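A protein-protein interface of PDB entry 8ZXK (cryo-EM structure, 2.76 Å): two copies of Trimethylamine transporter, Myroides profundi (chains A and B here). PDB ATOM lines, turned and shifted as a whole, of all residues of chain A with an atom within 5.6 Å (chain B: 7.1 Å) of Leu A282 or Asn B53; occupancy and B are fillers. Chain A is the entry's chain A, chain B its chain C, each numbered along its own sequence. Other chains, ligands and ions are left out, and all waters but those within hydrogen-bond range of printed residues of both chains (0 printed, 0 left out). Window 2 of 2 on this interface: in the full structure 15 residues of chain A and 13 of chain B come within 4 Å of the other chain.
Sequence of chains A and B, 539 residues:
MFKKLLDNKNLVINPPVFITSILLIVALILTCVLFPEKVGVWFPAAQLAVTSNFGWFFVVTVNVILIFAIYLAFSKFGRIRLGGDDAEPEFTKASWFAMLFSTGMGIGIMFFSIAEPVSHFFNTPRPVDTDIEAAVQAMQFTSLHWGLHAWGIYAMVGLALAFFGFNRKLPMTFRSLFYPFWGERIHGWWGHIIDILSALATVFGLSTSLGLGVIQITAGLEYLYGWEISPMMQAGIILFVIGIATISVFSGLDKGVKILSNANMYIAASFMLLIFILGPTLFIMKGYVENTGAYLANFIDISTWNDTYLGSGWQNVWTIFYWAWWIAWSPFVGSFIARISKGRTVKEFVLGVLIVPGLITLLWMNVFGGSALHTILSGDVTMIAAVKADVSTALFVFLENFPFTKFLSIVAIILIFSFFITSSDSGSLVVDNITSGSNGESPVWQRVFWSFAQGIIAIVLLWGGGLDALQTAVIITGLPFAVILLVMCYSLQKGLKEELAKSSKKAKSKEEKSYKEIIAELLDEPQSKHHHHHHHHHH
O of Lys A286 sits at hydrogen-bond distance from OG1 of Thr B308.
O of Leu B48 is in hydrogen-bond range of OG of Ser B52, at 3.2 Å.
The backbone carbonyl oxygen of Asn B53 sits at hydrogen-bond distance from the indole nitrogen of Trp B56 (2.8 Å).
Among the printed residues, pairs that only touch across the chains: Leu A282 with Ser B52, Leu A282 with Asn B53, Leu A282 with Trp B56, Phe A283 with Thr B308, Met A285 with Trp B56, Lys A286 with Trp B56 and Gly A287 with Thr B308.
Leu A282 touches just these residues of chain B: Ser B52, Asn B53 and Trp B56.
Of chain A, only Leu A282 (3.9 Å) comes within 4 Å of Asn B53.
Printed residues of chain B within 4 Å of Gly A287: Thr B308.
Printed residues of chain A within 4 Å of Ser B52: Leu A282 (3.3 Å).
The nearest printed residue of chain A that does not touch Asn B53 is Lys A286 (6.8 Å).
The nearest printed residue of chain A that does not touch Trp B56 is Thr A281 (6.5 Å).
Of the 14 printed residues of chain B, 4 touch a printed residue of chain A.
Hydrophobic or aromatic side chains of chain B within 4 Å of the printed part of chain A: Trp B56.
No position is printed for both chains.
Of the 8 pairs that touch across the chains among the printed residues, none has its exchanged pair printed and touching as well.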
ATOM      1  N   PRO A 280      10.974   8.402  14.162  1.00  0.00           N
ATOM      2  CA  PRO A 280       9.907   9.396  14.333  1.00  0.00           C
ATOM      3  C   PRO A 280       8.969   9.012  15.466  1.00  0.00           C
ATOM      4  O   PRO A 280       8.091   8.165  15.293  1.00  0.00           O
ATOM      5  CB  PRO A 280       9.197   9.387  12.975  1.00  0.00           C
ATOM      6  CG  PRO A 280       9.462   8.029  12.419  1.00  0.00           C
ATOM      7  CD  PRO A 280      10.780   7.564  12.966  1.00  0.00           C
ATOM      8  N   THR A 281       9.125   9.663  16.619  1.00  0.00           N
ATOM      9  CA  THR A 281       8.399   9.247  17.815  1.00  0.00           C
ATOM     10  C   THR A 281       6.910   9.544  17.693  1.00  0.00           C
ATOM     11  O   THR A 281       6.066   8.676  17.958  1.00  0.00           O
ATOM     12  CB  THR A 281       8.989   9.941  19.044  1.00  0.00           C
ATOM     13  OG1 THR A 281      10.272   9.379  19.340  1.00  0.00           O
ATOM     14  CG2 THR A 281       8.080   9.774  20.244  1.00  0.00           C
ATOM     15  N   LEU A 282       6.567  10.769  17.288  1.00  0.00           N
ATOM     16  CA  LEU A 282       5.164  11.133  17.137  1.00  0.00           C
ATOM     17  C   LEU A 282       4.495  10.291  16.060  1.00  0.00           C
ATOM     18  O   LEU A 282       3.355   9.839  16.233  1.00  0.00           O
ATOM     19  CB  LEU A 282       5.047  12.621  16.812  1.00  0.00           C
ATOM     20  CG  LEU A 282       3.641  13.149  16.532  1.00  0.00           C
ATOM     21  CD1 LEU A 282       2.780  13.041  17.776  1.00  0.00           C
ATOM     22  CD2 LEU A 282       3.710  14.583  16.040  1.00  0.00           C
ATOM     23  N   PHE A 283       5.191  10.070  14.943  1.00  0.00           N
ATOM     24  CA  PHE A 283       4.645   9.214  13.898  1.00  0.00           C
ATOM     25  C   PHE A 283       4.426   7.801  14.413  1.00  0.00           C
ATOM     26  O   PHE A 283       3.408   7.179  14.103  1.00  0.00           O
ATOM     27  CB  PHE A 283       5.565   9.199  12.678  1.00  0.00           C
ATOM     28  CG  PHE A 283       5.032   8.383  11.530  1.00  0.00           C
ATOM     29  CD1 PHE A 283       5.292   7.025  11.444  1.00  0.00           C
ATOM     30  CD2 PHE A 283       4.269   8.975  10.540  1.00  0.00           C
ATOM     31  CE1 PHE A 283       4.797   6.275  10.398  1.00  0.00           C
ATOM     32  CE2 PHE A 283       3.775   8.229   9.488  1.00  0.00           C
ATOM     33  CZ  PHE A 283       4.040   6.878   9.417  1.00  0.00           C
ATOM     34  N   ILE A 284       5.369   7.273  15.196  1.00  0.00           N
ATOM     35  CA  ILE A 284       5.214   5.913  15.706  1.00  0.00           C
ATOM     36  C   ILE A 284       4.013   5.824  16.638  1.00  0.00           C
ATOM     37  O   ILE A 284       3.237   4.869  16.570  1.00  0.00           O
ATOM     38  CB  ILE A 284       6.503   5.433  16.397  1.00  0.00           C
ATOM     39  CG1 ILE A 284       7.588   5.137  15.364  1.00  0.00           C
ATOM     40  CG2 ILE A 284       6.227   4.178  17.201  1.00  0.00           C
ATOM     41  CD1 ILE A 284       8.981   5.108  15.941  1.00  0.00           C
ATOM     42  N   MET A 285       3.833   6.812  17.518  1.00  0.00           N
ATOM     43  CA  MET A 285       2.698   6.771  18.439  1.00  0.00           C
ATOM     44  C   MET A 285       1.369   6.867  17.693  1.00  0.00           C
ATOM     45  O   MET A 285       0.446   6.069  17.928  1.00  0.00           O
ATOM     46  CB  MET A 285       2.816   7.895  19.468  1.00  0.00           C
ATOM     47  CG  MET A 285       3.614   7.522  20.706  1.00  0.00           C
ATOM     48  SD  MET A 285       3.181   5.901  21.364  1.00  0.00           S
ATOM     49  CE  MET A 285       1.485   6.171  21.866  1.00  0.00           C
ATOM     50  N   LYS A 286       1.254   7.844  16.787  1.00  0.00           N
ATOM     51  CA  LYS A 286       0.021   8.000  16.024  1.00  0.00           C
ATOM     52  C   LYS A 286      -0.257   6.768  15.176  1.00  0.00           C
ATOM     53  O   LYS A 286      -1.400   6.308  15.094  1.00  0.00           O
ATOM     54  CB  LYS A 286       0.104   9.245  15.142  1.00  0.00           C
ATOM     55  CG  LYS A 286       0.232  10.546  15.908  1.00  0.00           C
ATOM     56  CD  LYS A 286      -0.389  11.695  15.136  1.00  0.00           C
ATOM     57  CE  LYS A 286       0.242  11.842  13.767  1.00  0.00           C
ATOM     58  NZ  LYS A 286      -0.401  12.925  12.976  1.00  0.00           N
ATOM     59  N   GLY A 287       0.779   6.224  14.535  1.00  0.00           N
ATOM     60  CA  GLY A 287       0.601   5.032  13.733  1.00  0.00           C
ATOM     61  C   GLY A 287       0.235   3.822  14.562  1.00  0.00           C
ATOM     62  O   GLY A 287      -0.559   2.994  14.131  1.00  0.00           O
ATOM     63  N   GLN B  47      -1.269  26.248  20.364  1.00  0.00           N
ATOM     64  CA  GLN B  47      -2.348  25.333  20.007  1.00  0.00           C
ATOM     65  C   GLN B  47      -1.888  24.315  18.975  1.00  0.00           C
ATOM     66  O   GLN B  47      -2.200  23.123  19.087  1.00  0.00           O
ATOM     67  CB  GLN B  47      -3.554  26.112  19.485  1.00  0.00           C
ATOM     68  CG  GLN B  47      -4.657  25.226  18.930  1.00  0.00           C
ATOM     69  CD  GLN B  47      -5.643  25.985  18.066  1.00  0.00           C
ATOM     70  OE1 GLN B  47      -5.615  27.213  18.004  1.00  0.00           O
ATOM     71  NE2 GLN B  47      -6.523  25.254  17.395  1.00  0.00           N
ATOM     72  N   LEU B  48      -1.141  24.762  17.962  1.00  0.00           N
ATOM     73  CA  LEU B  48      -0.641  23.844  16.948  1.00  0.00           C
ATOM     74  C   LEU B  48       0.303  22.819  17.560  1.00  0.00           C
ATOM     75  O   LEU B  48       0.224  21.627  17.242  1.00  0.00           O
ATOM     76  CB  LEU B  48       0.053  24.629  15.833  1.00  0.00           C
ATOM     77  CG  LEU B  48       0.584  23.907  14.590  1.00  0.00           C
ATOM     78  CD1 LEU B  48       2.025  23.444  14.775  1.00  0.00           C
ATOM     79  CD2 LEU B  48      -0.318  22.745  14.197  1.00  0.00           C
ATOM     80  N   ALA B  49       1.198  23.261  18.446  1.00  0.00           N
ATOM     81  CA  ALA B  49       2.121  22.335  19.092  1.00  0.00           C
ATOM     82  C   ALA B  49       1.370  21.301  19.919  1.00  0.00           C
ATOM     83  O   ALA B  49       1.641  20.097  19.823  1.00  0.00           O
ATOM     84  CB  ALA B  49       3.113  23.106  19.962  1.00  0.00           C
ATOM     85  N   VAL B  50       0.406  21.751  20.726  1.00  0.00           N
ATOM     86  CA  VAL B  50      -0.336  20.830  21.583  1.00  0.00           C
ATOM     87  C   VAL B  50      -1.112  19.827  20.739  1.00  0.00           C
ATOM     88  O   VAL B  50      -1.075  18.618  20.993  1.00  0.00           O
ATOM     89  CB  VAL B  50      -1.264  21.607  22.533  1.00  0.00           C
ATOM     90  CG1 VAL B  50      -2.239  20.660  23.209  1.00  0.00           C
ATOM     91  CG2 VAL B  50      -0.452  22.356  23.572  1.00  0.00           C
ATOM     92  N   THR B  51      -1.814  20.312  19.711  1.00  0.00           N
ATOM     93  CA  THR B  51      -2.602  19.418  18.869  1.00  0.00           C
ATOM     94  C   THR B  51      -1.711  18.412  18.155  1.00  0.00           C
ATOM     95  O   THR B  51      -1.963  17.204  18.204  1.00  0.00           O
ATOM     96  CB  THR B  51      -3.417  20.226  17.861  1.00  0.00           C
ATOM     97  OG1 THR B  51      -2.638  21.333  17.394  1.00  0.00           O
ATOM     98  CG2 THR B  51      -4.689  20.749  18.504  1.00  0.00           C
ATOM     99  N   SER B  52      -0.637  18.887  17.520  1.00  0.00           N
ATOM    100  CA  SER B  52       0.240  17.995  16.771  1.00  0.00           C
ATOM    101  C   SER B  52       0.877  16.948  17.674  1.00  0.00           C
ATOM    102  O   SER B  52       0.962  15.772  17.304  1.00  0.00           O
ATOM    103  CB  SER B  52       1.316  18.805  16.051  1.00  0.00           C
ATOM    104  OG  SER B  52       0.781  19.471  14.921  1.00  0.00           O
ATOM    105  N   ASN B  53       1.327  17.349  18.863  1.00  0.00           N
ATOM    106  CA  ASN B  53       2.057  16.434  19.726  1.00  0.00           C
ATOM    107  C   ASN B  53       1.163  15.560  20.595  1.00  0.00           C
ATOM    108  O   ASN B  53       1.652  14.570  21.149  1.00  0.00           O
ATOM    109  CB  ASN B  53       3.016  17.217  20.627  1.00  0.00           C
ATOM    110  CG  ASN B  53       4.261  17.668  19.894  1.00  0.00           C
ATOM    111  OD1 ASN B  53       4.328  17.610  18.668  1.00  0.00           O
ATOM    112  ND2 ASN B  53       5.256  18.122  20.645  1.00  0.00           N
ATOM    113  N   PHE B  54      -0.132  15.883  20.730  1.00  0.00           N
ATOM    114  CA  PHE B  54      -0.968  15.101  21.632  1.00  0.00           C
ATOM    115  C   PHE B  54      -2.345  14.779  21.056  1.00  0.00           C
ATOM    116  O   PHE B  54      -3.269  14.477  21.822  1.00  0.00           O
ATOM    117  CB  PHE B  54      -1.127  15.828  22.968  1.00  0.00           C
ATOM    118  CG  PHE B  54       0.178  16.162  23.631  1.00  0.00           C
ATOM    119  CD1 PHE B  54       0.950  15.170  24.210  1.00  0.00           C
ATOM    120  CD2 PHE B  54       0.638  17.467  23.668  1.00  0.00           C
ATOM    121  CE1 PHE B  54       2.153  15.473  24.816  1.00  0.00           C
ATOM    122  CE2 PHE B  54       1.840  17.776  24.274  1.00  0.00           C
ATOM    123  CZ  PHE B  54       2.598  16.777  24.847  1.00  0.00           C
ATOM    124  N   GLY B  55      -2.515  14.824  19.734  1.00  0.00           N
ATOM    125  CA  GLY B  55      -3.749  14.325  19.156  1.00  0.00           C
ATOM    126  C   GLY B  55      -3.944  12.846  19.412  1.00  0.00           C
ATOM    127  O   GLY B  55      -5.061  12.392  19.677  1.00  0.00           O
ATOM    128  N   TRP B  56      -2.858  12.074  19.342  1.00  0.00           N
ATOM    129  CA  TRP B  56      -2.930  10.659  19.679  1.00  0.00           C
ATOM    130  C   TRP B  56      -3.368  10.469  21.124  1.00  0.00           C
ATOM    131  O   TRP B  56      -4.154   9.567  21.428  1.00  0.00           O
ATOM    132  CB  TRP B  56      -1.576   9.991  19.432  1.00  0.00           C
ATOM    133  CG  TRP B  56      -0.471  10.565  20.264  1.00  0.00           C
ATOM    134  CD1 TRP B  56       0.342  11.607  19.936  1.00  0.00           C
ATOM    135  CD2 TRP B  56      -0.061  10.131  21.566  1.00  0.00           C
ATOM    136  NE1 TRP B  56       1.232  11.851  20.953  1.00  0.00           N
ATOM    137  CE2 TRP B  56       1.005  10.958  21.965  1.00  0.00           C
ATOM    138  CE3 TRP B  56      -0.494   9.124  22.434  1.00  0.00           C
ATOM    139  CZ2 TRP B  56       1.645  10.809  23.191  1.00  0.00           C
ATOM    140  CZ3 TRP B  56       0.141   8.979  23.651  1.00  0.00           C
ATOM    141  CH2 TRP B  56       1.200   9.816  24.018  1.00  0.00           C
ATOM    142  N   PHE B  57      -2.880  11.321  22.028  1.00  0.00           N
ATOM    143  CA  PHE B  57      -3.259  11.195  23.430  1.00  0.00           C
ATOM    144  C   PHE B  57      -4.719  11.567  23.647  1.00  0.00           C
ATOM    145  O   PHE B  57      -5.409  10.929  24.445  1.00  0.00           O
ATOM    146  CB  PHE B  57      -2.361  12.056  24.311  1.00  0.00           C
ATOM    147  CG  PHE B  57      -2.706  11.974  25.766  1.00  0.00           C
ATOM    148  CD1 PHE B  57      -2.639  10.765  26.437  1.00  0.00           C
ATOM    149  CD2 PHE B  57      -3.122  13.097  26.460  1.00  0.00           C
ATOM    150  CE1 PHE B  57      -2.965  10.678  27.772  1.00  0.00           C
ATOM    151  CE2 PHE B  57      -3.451  13.015  27.795  1.00  0.00           C
ATOM    152  CZ  PHE B  57      -3.371  11.803  28.451  1.00  0.00           C
ATOM    153  N   THR B 308      -2.265   9.700  10.336  1.00  0.00           N
ATOM    154  CA  THR B 308      -0.836   9.455  10.503  1.00  0.00           C
ATOM    155  C   THR B 308      -0.078   9.611   9.191  1.00  0.00           C
ATOM    156  O   THR B 308       0.964  10.274   9.139  1.00  0.00           O
ATOM    157  CB  THR B 308      -0.613   8.057  11.078  1.00  0.00           C
ATOM    158  OG1 THR B 308      -1.453   7.870  12.222  1.00  0.00           O
ATOM    159  CG2 THR B 308       0.835   7.876  11.483  1.00  0.00           C
ATOM    160  N   ASN B 316      -6.317  18.884  13.864  1.00  0.00           N
ATOM    161  CA  ASN B 316      -5.918  19.961  14.764  1.00  0.00           C
ATOM    162  C   ASN B 316      -7.033  20.977  14.960  1.00  0.00           C
ATOM    163  O   ASN B 316      -7.089  21.644  16.000  1.00  0.00           O
ATOM    164  CB  ASN B 316      -4.661  20.649  14.232  1.00  0.00           C
ATOM    165  CG  ASN B 316      -3.534  19.675  13.966  1.00  0.00           C
ATOM    166  OD1 ASN B 316      -3.661  18.478  14.224  1.00  0.00           O
ATOM    167  ND2 ASN B 316      -2.424  20.181  13.447  1.00  0.00           N
ATOM    168  N   LEU B 479      -5.995  19.484  27.677  1.00  0.00           N
ATOM    169  CA  LEU B 479      -4.960  18.447  27.712  1.00  0.00           C
ATOM    170  C   LEU B 479      -4.661  17.959  29.132  1.00  0.00           C
ATOM    171  O   LEU B 479      -4.848  16.754  29.414  1.00  0.00           O
ATOM    172  CB  LEU B 479      -3.708  18.952  26.987  1.00  0.00           C
ATOM    173  CG  LEU B 479      -2.475  18.050  27.015  1.00  0.00           C
ATOM    174  CD1 LEU B 479      -2.697  16.807  26.171  1.00  0.00           C
ATOM    175  CD2 LEU B 479      -1.249  18.811  26.543  1.00  0.00           C
